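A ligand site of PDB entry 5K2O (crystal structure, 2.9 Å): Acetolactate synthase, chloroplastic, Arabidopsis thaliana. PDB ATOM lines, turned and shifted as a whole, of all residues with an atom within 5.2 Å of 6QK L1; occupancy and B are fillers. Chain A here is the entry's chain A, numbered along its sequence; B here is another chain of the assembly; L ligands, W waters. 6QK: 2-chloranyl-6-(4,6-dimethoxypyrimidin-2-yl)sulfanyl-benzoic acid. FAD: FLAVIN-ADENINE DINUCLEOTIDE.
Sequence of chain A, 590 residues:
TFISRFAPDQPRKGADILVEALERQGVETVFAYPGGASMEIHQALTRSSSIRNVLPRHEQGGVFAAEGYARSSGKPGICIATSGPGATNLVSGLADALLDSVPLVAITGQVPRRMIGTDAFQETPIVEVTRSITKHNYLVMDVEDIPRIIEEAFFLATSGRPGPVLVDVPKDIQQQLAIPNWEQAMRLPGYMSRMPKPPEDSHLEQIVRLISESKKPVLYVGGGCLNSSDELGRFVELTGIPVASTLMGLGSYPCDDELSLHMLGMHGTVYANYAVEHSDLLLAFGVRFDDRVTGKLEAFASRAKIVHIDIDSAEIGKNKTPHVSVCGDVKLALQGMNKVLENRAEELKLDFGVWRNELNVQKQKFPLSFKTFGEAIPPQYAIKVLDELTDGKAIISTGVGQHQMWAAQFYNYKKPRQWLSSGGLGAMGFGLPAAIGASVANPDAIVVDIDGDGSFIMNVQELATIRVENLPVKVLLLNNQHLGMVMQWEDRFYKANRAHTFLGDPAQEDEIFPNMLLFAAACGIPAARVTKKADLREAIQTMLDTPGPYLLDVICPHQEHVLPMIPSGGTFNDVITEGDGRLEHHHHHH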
ATOM      1  N   MET A 266      36.487 -16.907  -7.108  1.00  0.00           N
ATOM      2  CA  MET A 266      35.634 -16.205  -8.077  1.00  0.00           C
ATOM      3  C   MET A 266      35.573 -14.711  -7.818  1.00  0.00           C
ATOM      4  O   MET A 266      35.754 -13.904  -8.719  1.00  0.00           O
ATOM      5  CB  MET A 266      34.226 -16.802  -8.076  1.00  0.00           C
ATOM      6  CG  MET A 266      33.241 -16.075  -8.968  1.00  0.00           C
ATOM      7  SD  MET A 266      31.673 -16.944  -9.146  1.00  0.00           S
ATOM      8  CE  MET A 266      32.128 -18.236 -10.300  1.00  0.00           C
ATOM      9  N   ASP A 291      35.150 -25.523  -6.952  1.00  0.00           N
ATOM     10  CA  ASP A 291      35.090 -24.931  -8.281  1.00  0.00           C
ATOM     11  C   ASP A 291      34.997 -23.405  -8.219  1.00  0.00           C
ATOM     12  O   ASP A 291      35.440 -22.705  -9.125  1.00  0.00           O
ATOM     13  CB  ASP A 291      33.899 -25.499  -9.059  1.00  0.00           C
ATOM     14  CG  ASP A 291      33.783 -24.933 -10.457  1.00  0.00           C
ATOM     15  OD1 ASP A 291      34.822 -24.789 -11.134  1.00  0.00           O
ATOM     16  OD2 ASP A 291      32.645 -24.627 -10.878  1.00  0.00           O
ATOM     17  N   ARG A 292      34.424 -22.902  -7.127  1.00  0.00           N
ATOM     18  CA  ARG A 292      34.277 -21.468  -6.910  1.00  0.00           C
ATOM     19  C   ARG A 292      35.619 -20.820  -6.588  1.00  0.00           C
ATOM     20  O   ARG A 292      35.786 -19.605  -6.716  1.00  0.00           O
ATOM     21  CB  ARG A 292      33.269 -21.187  -5.793  1.00  0.00           C
ATOM     22  CG  ARG A 292      31.826 -21.395  -6.216  1.00  0.00           C
ATOM     23  CD  ARG A 292      31.453 -20.381  -7.284  1.00  0.00           C
ATOM     24  NE  ARG A 292      30.452 -20.890  -8.208  1.00  0.00           N
ATOM     25  CZ  ARG A 292      30.719 -21.728  -9.203  1.00  0.00           C
ATOM     26  NH1 ARG A 292      31.946 -22.169  -9.393  1.00  0.00           N
ATOM     27  NH2 ARG A 292      29.749 -22.129 -10.008  1.00  0.00           N
ATOM     28  N   MET A 485      22.799 -10.437  -6.728  1.00  0.00           N
ATOM     29  CA  MET A 485      23.788 -11.273  -7.413  1.00  0.00           C
ATOM     30  C   MET A 485      23.246 -11.857  -8.709  1.00  0.00           C
ATOM     31  O   MET A 485      23.965 -11.974  -9.703  1.00  0.00           O
ATOM     32  CB  MET A 485      24.268 -12.402  -6.483  1.00  0.00           C
ATOM     33  CG  MET A 485      25.345 -13.289  -7.096  1.00  0.00           C
ATOM     34  SD  MET A 485      26.843 -12.408  -7.569  1.00  0.00           S
ATOM     35  CE  MET A 485      27.413 -11.807  -5.975  1.00  0.00           C
ATOM     36  N   VAL A 486      21.964 -12.211  -8.710  1.00  0.00           N
ATOM     37  CA  VAL A 486      21.314 -12.714  -9.910  1.00  0.00           C
ATOM     38  C   VAL A 486      21.205 -11.568 -10.910  1.00  0.00           C
ATOM     39  O   VAL A 486      21.368 -11.750 -12.115  1.00  0.00           O
ATOM     40  CB  VAL A 486      19.916 -13.303  -9.620  1.00  0.00           C
ATOM     41  CG1 VAL A 486      19.299 -13.878 -10.883  1.00  0.00           C
ATOM     42  CG2 VAL A 486      20.012 -14.365  -8.539  1.00  0.00           C
ATOM     43  N   TRP A 489      24.586 -11.073 -12.658  1.00  0.00           N
ATOM     44  CA  TRP A 489      24.780 -12.051 -13.726  1.00  0.00           C
ATOM     45  C   TRP A 489      23.933 -11.722 -14.951  1.00  0.00           C
ATOM     46  O   TRP A 489      24.339 -11.982 -16.076  1.00  0.00           O
ATOM     47  CB  TRP A 489      24.475 -13.460 -13.216  1.00  0.00           C
ATOM     48  CG  TRP A 489      25.592 -14.069 -12.428  1.00  0.00           C
ATOM     49  CD1 TRP A 489      26.209 -13.533 -11.341  1.00  0.00           C
ATOM     50  CD2 TRP A 489      26.213 -15.343 -12.662  1.00  0.00           C
ATOM     51  NE1 TRP A 489      27.188 -14.385 -10.883  1.00  0.00           N
ATOM     52  CE2 TRP A 489      27.206 -15.502 -11.679  1.00  0.00           C
ATOM     53  CE3 TRP A 489      26.029 -16.347 -13.606  1.00  0.00           C
ATOM     54  CZ2 TRP A 489      28.017 -16.635 -11.615  1.00  0.00           C
ATOM     55  CZ3 TRP A 489      26.827 -17.474 -13.545  1.00  0.00           C
ATOM     56  CH2 TRP A 489      27.814 -17.611 -12.557  1.00  0.00           C
ATOM     57  N   SER A 568      32.344 -18.234 -14.397  1.00  0.00           N
ATOM     58  CA  SER A 568      32.223 -19.668 -14.136  1.00  0.00           C
ATOM     59  C   SER A 568      33.143 -20.488 -15.037  1.00  0.00           C
ATOM     60  O   SER A 568      33.146 -20.311 -16.253  1.00  0.00           O
ATOM     61  CB  SER A 568      30.782 -20.123 -14.319  1.00  0.00           C
ATOM     62  OG  SER A 568      30.596 -21.440 -13.803  1.00  0.00           O
ATOM     63  N   GLY B  35      17.542 -18.294  -9.468  1.00  0.00           N
ATOM     64  CA  GLY B  35      18.847 -18.559  -8.890  1.00  0.00           C
ATOM     65  C   GLY B  35      19.780 -18.871 -10.036  1.00  0.00           C
ATOM     66  O   GLY B  35      19.339 -19.094 -11.159  1.00  0.00           O
ATOM     67  N   GLY B  36      21.081 -18.888  -9.761  1.00  0.00           N
ATOM     68  CA  GLY B  36      22.087 -19.092 -10.795  1.00  0.00           C
ATOM     69  C   GLY B  36      21.871 -20.336 -11.637  1.00  0.00           C
ATOM     70  O   GLY B  36      22.123 -20.329 -12.842  1.00  0.00           O
ATOM     71  N   ALA B  37      21.392 -21.405 -11.000  1.00  0.00           N
ATOM     72  CA  ALA B  37      21.227 -22.676 -11.686  1.00  0.00           C
ATOM     73  C   ALA B  37      19.948 -22.745 -12.517  1.00  0.00           C
ATOM     74  O   ALA B  37      19.739 -23.698 -13.258  1.00  0.00           O
ATOM     75  CB  ALA B  37      21.251 -23.814 -10.684  1.00  0.00           C
ATOM     76  N   MET B  39      18.681 -19.598 -14.007  1.00  0.00           N
ATOM     77  CA  MET B  39      18.594 -18.313 -14.690  1.00  0.00           C
ATOM     78  C   MET B  39      18.139 -18.458 -16.135  1.00  0.00           C
ATOM     79  O   MET B  39      17.309 -17.686 -16.614  1.00  0.00           O
ATOM     80  CB  MET B  39      19.931 -17.584 -14.648  1.00  0.00           C
ATOM     81  CG  MET B  39      20.264 -16.963 -13.304  1.00  0.00           C
ATOM     82  SD  MET B  39      21.706 -15.888 -13.375  1.00  0.00           S
ATOM     83  CE  MET B  39      21.096 -14.572 -14.425  1.00  0.00           C
ATOM     84  N   SER B  83      18.858 -24.626  -7.932  1.00  0.00           N
ATOM     85  CA  SER B  83      19.488 -25.775  -7.308  1.00  0.00           C
ATOM     86  C   SER B  83      19.700 -25.550  -5.818  1.00  0.00           C
ATOM     87  O   SER B  83      19.528 -24.445  -5.320  1.00  0.00           O
ATOM     88  CB  SER B  83      20.822 -26.091  -7.978  1.00  0.00           C
ATOM     89  OG  SER B  83      21.751 -25.045  -7.758  1.00  0.00           O
ATOM     90  N   VAL B 111      23.123 -28.279 -10.909  1.00  0.00           N
ATOM     91  CA  VAL B 111      24.477 -28.000 -11.370  1.00  0.00           C
ATOM     92  C   VAL B 111      24.721 -28.730 -12.685  1.00  0.00           C
ATOM     93  O   VAL B 111      24.004 -29.687 -13.006  1.00  0.00           O
ATOM     94  CB  VAL B 111      25.529 -28.423 -10.314  1.00  0.00           C
ATOM     95  CG1 VAL B 111      25.266 -27.729  -8.991  1.00  0.00           C
ATOM     96  CG2 VAL B 111      25.524 -29.933 -10.139  1.00  0.00           C
ATOM     97  N   PRO B 112      25.720 -28.283 -13.475  1.00  0.00           N
ATOM     98  CA  PRO B 112      26.039 -28.985 -14.730  1.00  0.00           C
ATOM     99  C   PRO B 112      26.250 -30.485 -14.521  1.00  0.00           C
ATOM    100  O   PRO B 112      26.764 -30.890 -13.477  1.00  0.00           O
ATOM    101  CB  PRO B 112      27.336 -28.307 -15.174  1.00  0.00           C
ATOM    102  CG  PRO B 112      27.229 -26.931 -14.629  1.00  0.00           C
ATOM    103  CD  PRO B 112      26.512 -27.057 -13.312  1.00  0.00           C
ATOM    104  N   MET B 115      29.331 -32.025 -13.037  1.00  0.00           N
ATOM    105  CA  MET B 115      29.665 -31.615 -11.669  1.00  0.00           C
ATOM    106  C   MET B 115      28.780 -32.300 -10.623  1.00  0.00           C
ATOM    107  O   MET B 115      28.983 -32.117  -9.423  1.00  0.00           O
ATOM    108  CB  MET B 115      29.556 -30.104 -11.531  1.00  0.00           C
ATOM    109  CG  MET B 115      30.478 -29.331 -12.463  1.00  0.00           C
ATOM    110  SD  MET B 115      30.308 -27.545 -12.277  1.00  0.00           S
ATOM    111  CE  MET B 115      30.661 -27.367 -10.527  1.00  0.00           C
ATOM    112  N   PHE B 121      28.886 -26.169  -5.954  1.00  0.00           N
ATOM    113  CA  PHE B 121      28.190 -24.990  -5.441  1.00  0.00           C
ATOM    114  C   PHE B 121      26.680 -25.143  -5.594  1.00  0.00           C
ATOM    115  O   PHE B 121      26.187 -25.366  -6.700  1.00  0.00           O
ATOM    116  CB  PHE B 121      28.673 -23.724  -6.150  1.00  0.00           C
ATOM    117  CG  PHE B 121      27.995 -22.468  -5.687  1.00  0.00           C
ATOM    118  CD1 PHE B 121      28.098 -22.054  -4.368  1.00  0.00           C
ATOM    119  CD2 PHE B 121      27.247 -21.696  -6.563  1.00  0.00           C
ATOM    120  CE1 PHE B 121      27.474 -20.908  -3.934  1.00  0.00           C
ATOM    121  CE2 PHE B 121      26.621 -20.544  -6.142  1.00  0.00           C
ATOM    122  CZ  PHE B 121      26.739 -20.146  -4.818  1.00  0.00           C
ATOM    123  N   GLN B 122      25.973 -25.030  -4.473  1.00  0.00           N
ATOM    124  CA  GLN B 122      24.518 -25.157  -4.442  1.00  0.00           C
ATOM    125  C   GLN B 122      24.030 -26.463  -5.059  1.00  0.00           C
ATOM    126  O   GLN B 122      23.051 -26.483  -5.808  1.00  0.00           O
ATOM    127  CB  GLN B 122      23.874 -23.964  -5.161  1.00  0.00           C
ATOM    128  CG  GLN B 122      24.278 -22.621  -4.591  1.00  0.00           C
ATOM    129  CD  GLN B 122      23.392 -21.488  -5.074  1.00  0.00           C
ATOM    130  OE1 GLN B 122      23.119 -21.365  -6.265  1.00  0.00           O
ATOM    131  NE2 GLN B 122      22.939 -20.658  -4.142  1.00  0.00           N
ATOM    132  N   LYS B 171      22.134 -27.226 -15.439  1.00  0.00           N
ATOM    133  CA  LYS B 171      22.287 -25.942 -16.114  1.00  0.00           C
ATOM    134  C   LYS B 171      22.749 -26.082 -17.567  1.00  0.00           C
ATOM    135  O   LYS B 171      22.241 -25.378 -18.440  1.00  0.00           O
ATOM    136  CB  LYS B 171      23.254 -25.044 -15.346  1.00  0.00           C
ATOM    137  CG  LYS B 171      23.303 -23.618 -15.868  1.00  0.00           C
ATOM    138  CD  LYS B 171      24.180 -22.733 -15.010  1.00  0.00           C
ATOM    139  CE  LYS B 171      24.098 -21.287 -15.475  1.00  0.00           C
ATOM    140  NZ  LYS B 171      24.914 -20.372 -14.638  1.00  0.00           N
HETATM  141  C11 6QK L   1      27.484 -18.352  -8.576  1.00  0.00           C
HETATM  142 CL01 6QK L   1      28.473 -24.691 -11.589  1.00  0.00          CL
HETATM  143  C02 6QK L   1      27.194 -23.789 -10.818  1.00  0.00           C
HETATM  144  C03 6QK L   1      26.856 -22.535 -11.304  1.00  0.00           C
HETATM  145  C04 6QK L   1      27.582 -21.948 -12.492  1.00  0.00           C
HETATM  146  O05 6QK L   1      28.699 -21.388 -12.318  1.00  0.00           O
HETATM  147  O06 6QK L   1      27.083 -22.014 -13.650  1.00  0.00           O
HETATM  148  C07 6QK L   1      25.840 -21.818 -10.704  1.00  0.00           C
HETATM  149  S08 6QK L   1      25.419 -20.219 -11.337  1.00  0.00           S
HETATM  150  C09 6QK L   1      25.943 -18.988 -10.180  1.00  0.00           C
HETATM  151  N10 6QK L   1      27.033 -19.229  -9.479  1.00  0.00           N
HETATM  152  O12 6QK L   1      28.646 -18.626  -7.840  1.00  0.00           O
HETATM  153  C13 6QK L   1      28.803 -17.805  -6.707  1.00  0.00           C
HETATM  154  C14 6QK L   1      26.769 -17.150  -8.423  1.00  0.00           C
HETATM  155  C15 6QK L   1      25.616 -16.939  -9.203  1.00  0.00           C
HETATM  156  O16 6QK L   1      24.874 -15.754  -9.079  1.00  0.00           O
HETATM  157  C17 6QK L   1      23.539 -15.873  -9.528  1.00  0.00           C
HETATM  158  N18 6QK L   1      25.236 -17.883 -10.073  1.00  0.00           N
HETATM  159  C19 6QK L   1      25.165 -22.331  -9.615  1.00  0.00           C
HETATM  160  C20 6QK L   1      25.512 -23.580  -9.120  1.00  0.00           C
HETATM  161  C21 6QK L   1      26.522 -24.312  -9.726  1.00  0.00           C
HETATM  162  PA  FAD L   2      35.226 -26.138   3.520  1.00  0.00           P
HETATM  163  O1A FAD L   2      35.201 -25.026   4.575  1.00  0.00           O
HETATM  164  O2A FAD L   2      33.913 -26.162   2.768  1.00  0.00           O
HETATM  165  O5B FAD L   2      35.466 -27.549   4.246  1.00  0.00           O
HETATM  166  C5B FAD L   2      36.583 -27.669   5.156  1.00  0.00           C
HETATM  167  C4B FAD L   2      37.612 -28.605   4.532  1.00  0.00           C
HETATM  168  O4B FAD L   2      38.710 -28.803   5.419  1.00  0.00           O
HETATM  169  C3B FAD L   2      37.013 -29.952   4.310  1.00  0.00           C
HETATM  170  O3B FAD L   2      37.646 -30.585   3.195  1.00  0.00           O
HETATM  171  C2B FAD L   2      37.322 -30.679   5.547  1.00  0.00           C
HETATM  172  O2B FAD L   2      37.422 -32.095   5.291  1.00  0.00           O
HETATM  173  C1B FAD L   2      38.626 -30.147   5.959  1.00  0.00           C
HETATM  174  N9A FAD L   2      38.757 -30.103   7.356  1.00  0.00           N
HETATM  175  C8A FAD L   2      37.798 -29.852   8.236  1.00  0.00           C
HETATM  176  N7A FAD L   2      38.305 -29.881   9.472  1.00  0.00           N
HETATM  177  C5A FAD L   2      39.648 -30.148   9.390  1.00  0.00           C
HETATM  178  C6A FAD L   2      40.724 -30.308  10.317  1.00  0.00           C
HETATM  179  N6A FAD L   2      40.506 -30.182  11.688  1.00  0.00           N
HETATM  180  N1A FAD L   2      41.961 -30.576   9.845  1.00  0.00           N
HETATM  181  C2A FAD L   2      42.179 -30.700   8.557  1.00  0.00           C
HETATM  182  N3A FAD L   2      41.202 -30.558   7.652  1.00  0.00           N
HETATM  183  C4A FAD L   2      39.944 -30.291   8.029  1.00  0.00           C
HETATM  184  N1  FAD L   2      34.625 -19.263  -1.689  1.00  0.00           N
HETATM  185  C2  FAD L   2      35.899 -18.711  -1.979  1.00  0.00           C
HETATM  186  O2  FAD L   2      36.876 -19.138  -1.393  1.00  0.00           O
HETATM  187  N3  FAD L   2      36.038 -17.697  -2.906  1.00  0.00           N
HETATM  188  C4  FAD L   2      34.928 -17.212  -3.568  1.00  0.00           C
HETATM  189  O4  FAD L   2      35.041 -16.318  -4.393  1.00  0.00           O
HETATM  190  C4X FAD L   2      33.546 -17.787  -3.280  1.00  0.00           C
HETATM  191  N5  FAD L   2      32.400 -17.320  -3.930  1.00  0.00           N
HETATM  192  C5X FAD L   2      31.190 -17.589  -3.358  1.00  0.00           C
HETATM  193  C6  FAD L   2      30.054 -16.841  -3.707  1.00  0.00           C
HETATM  194  C7  FAD L   2      28.819 -17.132  -3.110  1.00  0.00           C
HETATM  195  C7M FAD L   2      27.570 -16.316  -3.485  1.00  0.00           C
HETATM  196  C8  FAD L   2      28.713 -18.153  -2.168  1.00  0.00           C
HETATM  197  C8M FAD L   2      27.351 -18.436  -1.520  1.00  0.00           C
HETATM  198  C9  FAD L   2      29.838 -18.902  -1.809  1.00  0.00           C
HETATM  199  C9A FAD L   2      31.083 -18.608  -2.406  1.00  0.00           C
HETATM  200  N10 FAD L   2      32.203 -19.341  -2.062  1.00  0.00           N
HETATM  201  C10 FAD L   2      33.439 -18.801  -2.351  1.00  0.00           C
HETATM  202  C1' FAD L   2      32.111 -20.371  -1.086  1.00  0.00           C
HETATM  203  C2' FAD L   2      32.395 -21.747  -1.743  1.00  0.00           C
HETATM  204  O2' FAD L   2      31.209 -22.225  -2.358  1.00  0.00           O
HETATM  205  C3' FAD L   2      32.880 -22.786  -0.650  1.00  0.00           C
HETATM  206  O3' FAD L   2      32.081 -22.675   0.444  1.00  0.00           O
HETATM  207  C4' FAD L   2      34.315 -22.550  -0.276  1.00  0.00           C
HETATM  208  O4' FAD L   2      35.056 -22.119  -1.422  1.00  0.00           O
HETATM  209  C5' FAD L   2      34.896 -23.850   0.208  1.00  0.00           C
HETATM  210  O5' FAD L   2      35.454 -23.668   1.485  1.00  0.00           O
HETATM  211  P   FAD L   2      36.768 -24.525   1.835  1.00  0.00           P
HETATM  212  O1P FAD L   2      37.508 -24.822   0.526  1.00  0.00           O
HETATM  213  O2P FAD L   2      37.661 -23.724   2.758  1.00  0.00           O
HETATM  214  O3P FAD L   2      36.410 -25.891   2.516  1.00  0.00           O
HETATM  215  O   HOH W   1      27.975 -22.735 -16.205  1.00  0.00           O
HETATM  216  O   HOH W   2      28.959 -14.680  -8.761  1.00  0.00           O
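NH1 of Arg 292 lies within salt-bridge range of OD2 of Asp 291 (3.0 Å).
O of Arg 292 is in hydrogen-bond range of N of Met 266, 2.8 Å away.
O of Gly 36 of chain B sits at hydrogen-bond distance from NZ of Lys 171 of chain B (3.3 Å).
The side-chain amino group (NZ) of Lys 171 of chain B lies within salt-bridge range of an oxygen (O06) of 6QK L1.
NE1 of Trp 489 lies within hydrogen-bond range of O16 of 6QK L1 (3.2 Å).
The guanidinium group (NH2) of Arg 292 is in salt-bridge range of an oxygen (O05) of 6QK L1 (2.6 Å).
N of Met 266 is in hydrogen-bond range of O4 of FAD L2, at 3.1 Å.
OG of Ser 568 sits at hydrogen-bond distance from O05 of 6QK L1 (2.4 Å).
An oxygen (O12) of 6QK L1 sits close to the side-chain sulfur (SD) of Met 266, at 3.7 Å.
O of Gly 36 of chain B lies close to S08 of 6QK L1.
Residues that only touch 6QK L1: Phe 121 of chain B (3.1 Å), Met 485 (3.2 Å), Met 115 of chain B (3.5 Å), Pro 112 of chain B (3.5 Å), Val 111 of chain B (3.7 Å) and Val 486 (3.9 Å).
12 residues have an atom within 4 Å of 6QK L1: Met 266, Arg 292, Met 485, Val 486, Trp 489, Ser 568, Gly 36 of chain B, Val 111 of chain B, Pro 112 of chain B, Met 115 of chain B, Phe 121 of chain B and Lys 171 of chain B.
Water W2 lies within hydrogen-bond range of NE1 of Trp 489 (2.8 Å), SD of Met 485 (3.3 Å) and SD of Met 266 (3.6 Å).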
